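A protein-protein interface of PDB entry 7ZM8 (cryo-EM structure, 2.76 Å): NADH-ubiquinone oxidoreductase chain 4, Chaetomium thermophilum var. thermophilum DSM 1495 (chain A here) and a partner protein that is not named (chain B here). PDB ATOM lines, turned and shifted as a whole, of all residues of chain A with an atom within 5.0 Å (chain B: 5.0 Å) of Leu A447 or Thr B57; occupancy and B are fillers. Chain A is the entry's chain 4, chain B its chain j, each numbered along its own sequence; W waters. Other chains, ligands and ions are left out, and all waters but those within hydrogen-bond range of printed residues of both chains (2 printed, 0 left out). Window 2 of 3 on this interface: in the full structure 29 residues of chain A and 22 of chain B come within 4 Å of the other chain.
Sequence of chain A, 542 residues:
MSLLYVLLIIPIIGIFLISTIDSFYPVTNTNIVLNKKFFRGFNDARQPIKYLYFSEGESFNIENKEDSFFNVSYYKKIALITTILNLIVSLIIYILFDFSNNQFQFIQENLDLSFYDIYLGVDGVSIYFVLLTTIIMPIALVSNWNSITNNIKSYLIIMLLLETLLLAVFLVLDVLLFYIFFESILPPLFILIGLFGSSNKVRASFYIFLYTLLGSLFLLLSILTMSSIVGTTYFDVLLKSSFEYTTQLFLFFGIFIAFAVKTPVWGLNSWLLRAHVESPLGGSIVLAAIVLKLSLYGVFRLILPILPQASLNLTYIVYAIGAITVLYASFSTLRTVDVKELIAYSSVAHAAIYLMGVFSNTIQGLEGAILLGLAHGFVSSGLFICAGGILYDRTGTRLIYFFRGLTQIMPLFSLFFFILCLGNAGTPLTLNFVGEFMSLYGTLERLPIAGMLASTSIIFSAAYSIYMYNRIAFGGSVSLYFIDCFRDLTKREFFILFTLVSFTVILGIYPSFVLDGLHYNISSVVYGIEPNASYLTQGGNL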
ATOM      1  N   TYR A 316     -19.185   3.731 -18.895  1.00  0.00           N
ATOM      2  CA  TYR A 316     -19.743   2.559 -18.235  1.00  0.00           C
ATOM      3  C   TYR A 316     -21.228   2.723 -17.950  1.00  0.00           C
ATOM      4  O   TYR A 316     -21.951   1.725 -17.867  1.00  0.00           O
ATOM      5  CB  TYR A 316     -18.964   2.263 -16.953  1.00  0.00           C
ATOM      6  CG  TYR A 316     -19.256   3.204 -15.815  1.00  0.00           C
ATOM      7  CD1 TYR A 316     -18.702   4.471 -15.778  1.00  0.00           C
ATOM      8  CD2 TYR A 316     -20.097   2.828 -14.784  1.00  0.00           C
ATOM      9  CE1 TYR A 316     -18.974   5.330 -14.744  1.00  0.00           C
ATOM     10  CE2 TYR A 316     -20.367   3.676 -13.750  1.00  0.00           C
ATOM     11  CZ  TYR A 316     -19.807   4.929 -13.734  1.00  0.00           C
ATOM     12  OH  TYR A 316     -20.076   5.787 -12.697  1.00  0.00           O
ATOM     13  N   TYR A 319     -22.653   2.075 -21.491  1.00  0.00           N
ATOM     14  CA  TYR A 319     -22.547   0.667 -21.852  1.00  0.00           C
ATOM     15  C   TYR A 319     -23.502  -0.192 -21.036  1.00  0.00           C
ATOM     16  O   TYR A 319     -24.025  -1.189 -21.538  1.00  0.00           O
ATOM     17  CB  TYR A 319     -21.109   0.196 -21.674  1.00  0.00           C
ATOM     18  CG  TYR A 319     -20.253   0.450 -22.887  1.00  0.00           C
ATOM     19  CD1 TYR A 319     -20.570   1.463 -23.780  1.00  0.00           C
ATOM     20  CD2 TYR A 319     -19.135  -0.320 -23.145  1.00  0.00           C
ATOM     21  CE1 TYR A 319     -19.798   1.701 -24.886  1.00  0.00           C
ATOM     22  CE2 TYR A 319     -18.355  -0.082 -24.249  1.00  0.00           C
ATOM     23  CZ  TYR A 319     -18.696   0.926 -25.118  1.00  0.00           C
ATOM     24  OH  TYR A 319     -17.924   1.162 -26.224  1.00  0.00           O
ATOM     25  N   THR A 443     -16.461  -2.018 -28.840  1.00  0.00           N
ATOM     26  CA  THR A 443     -17.137  -2.123 -27.520  1.00  0.00           C
ATOM     27  C   THR A 443     -16.303  -3.021 -26.592  1.00  0.00           C
ATOM     28  O   THR A 443     -16.086  -2.625 -25.442  1.00  0.00           O
ATOM     29  CB  THR A 443     -18.618  -2.497 -27.691  1.00  0.00           C
ATOM     30  OG1 THR A 443     -19.228  -1.549 -28.566  1.00  0.00           O
ATOM     31  CG2 THR A 443     -19.386  -2.556 -26.391  1.00  0.00           C
ATOM     32  N   LEU A 444     -15.836  -4.170 -27.086  1.00  0.00           N
ATOM     33  CA  LEU A 444     -14.993  -5.105 -26.288  1.00  0.00           C
ATOM     34  C   LEU A 444     -13.644  -4.475 -25.922  1.00  0.00           C
ATOM     35  O   LEU A 444     -13.154  -4.732 -24.831  1.00  0.00           O
ATOM     36  CB  LEU A 444     -14.811  -6.406 -27.081  1.00  0.00           C
ATOM     37  CG  LEU A 444     -14.306  -7.596 -26.271  1.00  0.00           C
ATOM     38  CD1 LEU A 444     -15.439  -8.564 -25.981  1.00  0.00           C
ATOM     39  CD2 LEU A 444     -13.172  -8.302 -26.996  1.00  0.00           C
ATOM     40  N   GLU A 445     -13.038  -3.722 -26.834  1.00  0.00           N
ATOM     41  CA  GLU A 445     -11.716  -3.097 -26.566  1.00  0.00           C
ATOM     42  C   GLU A 445     -11.862  -1.975 -25.528  1.00  0.00           C
ATOM     43  O   GLU A 445     -10.924  -1.801 -24.732  1.00  0.00           O
ATOM     44  CB  GLU A 445     -11.053  -2.630 -27.865  1.00  0.00           C
ATOM     45  CG  GLU A 445      -9.633  -2.135 -27.670  1.00  0.00           C
ATOM     46  CD  GLU A 445      -8.927  -1.683 -28.935  1.00  0.00           C
ATOM     47  OE1 GLU A 445      -7.686  -1.768 -28.980  1.00  0.00           O
ATOM     48  OE2 GLU A 445      -9.621  -1.242 -29.867  1.00  0.00           O
ATOM     49  N   ARG A 446     -12.999  -1.272 -25.511  1.00  0.00           N
ATOM     50  CA  ARG A 446     -13.227  -0.163 -24.542  1.00  0.00           C
ATOM     51  C   ARG A 446     -13.461  -0.746 -23.152  1.00  0.00           C
ATOM     52  O   ARG A 446     -12.581  -0.579 -22.298  1.00  0.00           O
ATOM     53  CB  ARG A 446     -14.438   0.675 -24.960  1.00  0.00           C
ATOM     54  CG  ARG A 446     -14.819   1.781 -23.989  1.00  0.00           C
ATOM     55  CD  ARG A 446     -13.780   2.873 -23.864  1.00  0.00           C
ATOM     56  NE  ARG A 446     -14.162   3.786 -22.799  1.00  0.00           N
ATOM     57  CZ  ARG A 446     -13.807   3.650 -21.530  1.00  0.00           C
ATOM     58  NH1 ARG A 446     -14.214   4.530 -20.635  1.00  0.00           N
ATOM     59  NH2 ARG A 446     -13.035   2.643 -21.162  1.00  0.00           N
ATOM     60  N   LEU A 447     -14.607  -1.374 -22.931  1.00  0.00           N
ATOM     61  CA  LEU A 447     -14.883  -2.071 -21.655  1.00  0.00           C
ATOM     62  C   LEU A 447     -15.234  -3.493 -22.051  1.00  0.00           C
ATOM     63  O   LEU A 447     -16.361  -3.708 -22.504  1.00  0.00           O
ATOM     64  CB  LEU A 447     -16.079  -1.372 -21.007  1.00  0.00           C
ATOM     65  CG  LEU A 447     -16.714  -2.082 -19.818  1.00  0.00           C
ATOM     66  CD1 LEU A 447     -15.767  -2.094 -18.629  1.00  0.00           C
ATOM     67  CD2 LEU A 447     -18.016  -1.397 -19.461  1.00  0.00           C
ATOM     68  N   PRO A 448     -14.335  -4.507 -21.971  1.00  0.00           N
ATOM     69  CA  PRO A 448     -14.647  -5.872 -22.401  1.00  0.00           C
ATOM     70  C   PRO A 448     -15.964  -6.503 -21.944  1.00  0.00           C
ATOM     71  O   PRO A 448     -16.590  -7.115 -22.773  1.00  0.00           O
ATOM     72  CB  PRO A 448     -13.508  -6.742 -21.867  1.00  0.00           C
ATOM     73  CG  PRO A 448     -12.327  -5.832 -21.826  1.00  0.00           C
ATOM     74  CD  PRO A 448     -12.901  -4.444 -21.660  1.00  0.00           C
ATOM     75  N   ILE A 449     -16.336  -6.367 -20.669  1.00  0.00           N
ATOM     76  CA  ILE A 449     -17.526  -7.124 -20.190  1.00  0.00           C
ATOM     77  C   ILE A 449     -18.777  -6.732 -20.965  1.00  0.00           C
ATOM     78  O   ILE A 449     -19.535  -7.621 -21.322  1.00  0.00           O
ATOM     79  CB  ILE A 449     -17.712  -6.983 -18.665  1.00  0.00           C
ATOM     80  CG1 ILE A 449     -17.898  -5.535 -18.205  1.00  0.00           C
ATOM     81  CG2 ILE A 449     -16.590  -7.681 -17.911  1.00  0.00           C
ATOM     82  CD1 ILE A 449     -19.303  -5.220 -17.746  1.00  0.00           C
ATOM     83  N   ALA A 450     -19.001  -5.449 -21.189  1.00  0.00           N
ATOM     84  CA  ALA A 450     -20.252  -5.017 -21.847  1.00  0.00           C
ATOM     85  C   ALA A 450     -20.281  -5.485 -23.291  1.00  0.00           C
ATOM     86  O   ALA A 450     -21.346  -5.923 -23.708  1.00  0.00           O
ATOM     87  CB  ALA A 450     -20.432  -3.529 -21.720  1.00  0.00           C
ATOM     88  N   GLY A 451     -19.160  -5.391 -24.015  1.00  0.00           N
ATOM     89  CA  GLY A 451     -19.128  -5.978 -25.342  1.00  0.00           C
ATOM     90  C   GLY A 451     -19.393  -7.468 -25.333  1.00  0.00           C
ATOM     91  O   GLY A 451     -19.841  -8.030 -26.334  1.00  0.00           O
ATOM     92  N   LEU B  53     -20.270  -3.833 -12.387  1.00  0.00           N
ATOM     93  CA  LEU B  53     -19.164  -4.572 -12.978  1.00  0.00           C
ATOM     94  C   LEU B  53     -18.475  -3.759 -14.061  1.00  0.00           C
ATOM     95  O   LEU B  53     -17.260  -3.872 -14.243  1.00  0.00           O
ATOM     96  CB  LEU B  53     -19.655  -5.904 -13.541  1.00  0.00           C
ATOM     97  CG  LEU B  53     -19.774  -7.098 -12.593  1.00  0.00           C
ATOM     98  CD1 LEU B  53     -18.406  -7.490 -12.056  1.00  0.00           C
ATOM     99  CD2 LEU B  53     -20.735  -6.840 -11.452  1.00  0.00           C
ATOM    100  N   ALA B  54     -19.237  -2.937 -14.779  1.00  0.00           N
ATOM    101  CA  ALA B  54     -18.657  -2.087 -15.808  1.00  0.00           C
ATOM    102  C   ALA B  54     -17.678  -1.092 -15.208  1.00  0.00           C
ATOM    103  O   ALA B  54     -16.666  -0.751 -15.829  1.00  0.00           O
ATOM    104  CB  ALA B  54     -19.770  -1.363 -16.563  1.00  0.00           C
ATOM    105  N   TYR B  55     -17.970  -0.605 -14.008  1.00  0.00           N
ATOM    106  CA  TYR B  55     -17.102   0.380 -13.375  1.00  0.00           C
ATOM    107  C   TYR B  55     -15.858  -0.275 -12.787  1.00  0.00           C
ATOM    108  O   TYR B  55     -14.756   0.280 -12.874  1.00  0.00           O
ATOM    109  CB  TYR B  55     -17.892   1.128 -12.305  1.00  0.00           C
ATOM    110  CG  TYR B  55     -17.089   2.127 -11.515  1.00  0.00           C
ATOM    111  CD1 TYR B  55     -16.934   3.424 -11.969  1.00  0.00           C
ATOM    112  CD2 TYR B  55     -16.496   1.778 -10.314  1.00  0.00           C
ATOM    113  CE1 TYR B  55     -16.208   4.341 -11.256  1.00  0.00           C
ATOM    114  CE2 TYR B  55     -15.767   2.688  -9.594  1.00  0.00           C
ATOM    115  CZ  TYR B  55     -15.627   3.969 -10.067  1.00  0.00           C
ATOM    116  OH  TYR B  55     -14.898   4.886  -9.348  1.00  0.00           O
ATOM    117  N   LYS B  56     -16.031  -1.452 -12.197  1.00  0.00           N
ATOM    118  CA  LYS B  56     -14.936  -2.125 -11.476  1.00  0.00           C
ATOM    119  C   LYS B  56     -13.887  -2.658 -12.435  1.00  0.00           C
ATOM    120  O   LYS B  56     -12.712  -2.723 -12.045  1.00  0.00           O
ATOM    121  CB  LYS B  56     -15.539  -3.257 -10.652  1.00  0.00           C
ATOM    122  CG  LYS B  56     -16.271  -2.808  -9.396  1.00  0.00           C
ATOM    123  CD  LYS B  56     -15.427  -1.951  -8.476  1.00  0.00           C
ATOM    124  CE  LYS B  56     -14.332  -2.730  -7.781  1.00  0.00           C
ATOM    125  NZ  LYS B  56     -13.485  -1.852  -6.939  1.00  0.00           N
ATOM    126  N   THR B  57     -14.307  -3.066 -13.622  1.00  0.00           N
ATOM    127  CA  THR B  57     -13.374  -3.705 -14.572  1.00  0.00           C
ATOM    128  C   THR B  57     -12.986  -2.726 -15.671  1.00  0.00           C
ATOM    129  O   THR B  57     -12.387  -3.179 -16.651  1.00  0.00           O
ATOM    130  CB  THR B  57     -14.021  -4.976 -15.125  1.00  0.00           C
ATOM    131  OG1 THR B  57     -15.149  -4.579 -15.900  1.00  0.00           O
ATOM    132  CG2 THR B  57     -14.456  -5.934 -14.040  1.00  0.00           C
ATOM    133  N   ASP B  58     -13.282  -1.439 -15.513  1.00  0.00           N
ATOM    134  CA  ASP B  58     -13.060  -0.469 -16.612  1.00  0.00           C
ATOM    135  C   ASP B  58     -11.583  -0.119 -16.683  1.00  0.00           C
ATOM    136  O   ASP B  58     -11.025   0.265 -15.663  1.00  0.00           O
ATOM    137  CB  ASP B  58     -13.960   0.749 -16.433  1.00  0.00           C
ATOM    138  CG  ASP B  58     -13.870   1.783 -17.539  1.00  0.00           C
ATOM    139  OD1 ASP B  58     -13.428   1.432 -18.648  1.00  0.00           O
ATOM    140  OD2 ASP B  58     -14.252   2.935 -17.274  1.00  0.00           O
ATOM    141  N   GLY B  59     -10.938  -0.345 -17.827  1.00  0.00           N
ATOM    142  CA  GLY B  59      -9.486  -0.114 -17.966  1.00  0.00           C
ATOM    143  C   GLY B  59      -8.660  -1.159 -17.240  1.00  0.00           C
ATOM    144  O   GLY B  59      -7.459  -0.935 -17.067  1.00  0.00           O
ATOM    145  N   LEU B  60      -9.294  -2.220 -16.751  1.00  0.00           N
ATOM    146  CA  LEU B  60      -8.574  -3.294 -16.019  1.00  0.00           C
ATOM    147  C   LEU B  60      -7.650  -4.084 -16.948  1.00  0.00           C
ATOM    148  O   LEU B  60      -6.561  -4.455 -16.501  1.00  0.00           O
ATOM    149  CB  LEU B  60      -9.582  -4.210 -15.323  1.00  0.00           C
ATOM    150  CG  LEU B  60      -9.012  -5.135 -14.251  1.00  0.00           C
ATOM    151  CD1 LEU B  60      -8.065  -4.383 -13.330  1.00  0.00           C
ATOM    152  CD2 LEU B  60     -10.130  -5.779 -13.450  1.00  0.00           C
ATOM    153  N   TRP B  61      -8.071  -4.355 -18.181  1.00  0.00           N
ATOM    154  CA  TRP B  61      -7.256  -5.239 -19.051  1.00  0.00           C
ATOM    155  C   TRP B  61      -6.977  -4.638 -20.427  1.00  0.00           C
ATOM    156  O   TRP B  61      -7.812  -3.847 -20.896  1.00  0.00           O
ATOM    157  CB  TRP B  61      -7.957  -6.591 -19.225  1.00  0.00           C
ATOM    158  CG  TRP B  61      -8.242  -7.334 -17.959  1.00  0.00           C
ATOM    159  CD1 TRP B  61      -7.337  -7.883 -17.099  1.00  0.00           C
ATOM    160  CD2 TRP B  61      -9.540  -7.643 -17.428  1.00  0.00           C
ATOM    161  NE1 TRP B  61      -7.984  -8.499 -16.062  1.00  0.00           N
ATOM    162  CE2 TRP B  61      -9.335  -8.369 -16.238  1.00  0.00           C
ATOM    163  CE3 TRP B  61     -10.849  -7.368 -17.837  1.00  0.00           C
ATOM    164  CZ2 TRP B  61     -10.394  -8.826 -15.457  1.00  0.00           C
ATOM    165  CZ3 TRP B  61     -11.895  -7.821 -17.065  1.00  0.00           C
ATOM    166  CH2 TRP B  61     -11.667  -8.537 -15.891  1.00  0.00           C
ATOM    167  N   ARG B  75      -3.990  -2.280 -14.518  1.00  0.00           N
ATOM    168  CA  ARG B  75      -4.060  -1.587 -13.245  1.00  0.00           C
ATOM    169  C   ARG B  75      -3.701  -2.523 -12.099  1.00  0.00           C
ATOM    170  O   ARG B  75      -3.134  -2.108 -11.088  1.00  0.00           O
ATOM    171  CB  ARG B  75      -5.466  -1.007 -13.065  1.00  0.00           C
ATOM    172  CG  ARG B  75      -5.878  -0.687 -11.643  1.00  0.00           C
ATOM    173  CD  ARG B  75      -7.121   0.187 -11.640  1.00  0.00           C
ATOM    174  NE  ARG B  75      -8.340  -0.566 -11.925  1.00  0.00           N
ATOM    175  CZ  ARG B  75      -8.998  -0.524 -13.079  1.00  0.00           C
ATOM    176  NH1 ARG B  75     -10.101  -1.235 -13.239  1.00  0.00           N
ATOM    177  NH2 ARG B  75      -8.554   0.228 -14.071  1.00  0.00           N
ATOM    178  OXT ARG B  75      -3.958  -3.725 -12.167  1.00  0.00           O
HETATM  179  O   HOH W   1     -14.570  -5.239 -18.667  1.00  0.00           O
HETATM  180  O   HOH W   2     -16.396   4.568 -18.389  1.00  0.00           O
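OD1 of Asp B58 is in salt-bridge range of NH2 of Arg A446.
The backbone carbonyl oxygen (O) of Asp B58 is in hydrogen-bond range of the guanidinium group (NH2) of Arg B75, at 2.9 Å. The side-chain hydroxyl (OG1) of Thr B57 is in hydrogen-bond range of the backbone carbonyl oxygen (O) of Leu B53 (2.8 Å).
Among the printed residues, pairs that only touch across the chains: Tyr A316 with Ala B54, Tyr A316 with Tyr B55, Leu A447 with Ala B54, Leu A447 with Thr B57, Leu A447 with Asp B58, Ile A449 with Ala B54 and Ile A449 with Thr B57.
Printed residues of chain B within 4 Å of Tyr A316: Ala B54 and Tyr B55. Of the printed residues of chain B, Arg A446 touches Asp B58. Of chain B, only Ala B54 (3.2 Å), Thr B57 (3.7 Å) and Asp B58 (3.7 Å) come within 4 Å of Leu A447. Thr B57 touches just these residues of chain A: Leu A447 (3.7 Å) and Ile A449 (3.7 Å). Of the printed residues of chain A, Asp B58 touches Arg A446 (2.8 Å) and Leu A447 (3.7 Å). The nearest printed residue of chain B that does not touch Tyr A316 is Asp B58 (4.8 Å).
Of the 11 printed residues of chain A, 4 touch a printed residue of chain B. Hydrophobic or aromatic side chains of chain A within 4 Å of the printed part of chain B: Tyr A316, Leu A447 and Ile A449. Of the 10 printed residues of chain B, 4 touch a printed residue of chain A. Hydrophobic or aromatic side chains of chain B that line the printed part of chain A: Ala B54 and Tyr B55. Along chain B the printed residues that touch a printed residue of chain A span positions 54 to 58. Among the printed residues, 8 pairs touch across the chains. Among the printed residues, Asp or Glu carboxylates within 4 Å of a Lys or Arg side-chain nitrogen of the other chain: Arg A446 with Asp B58.
Water W1 lies within hydrogen-bond range of N of Ile A449 (2.9 Å) and OG1 of Thr B57 (2.9 Å). Water W2 lies within hydrogen-bond range of the side-chain carboxylate (OD2) of Asp B58, the backbone NH (N) of Tyr A316 and the guanidinium group (NH1) of Arg A446.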
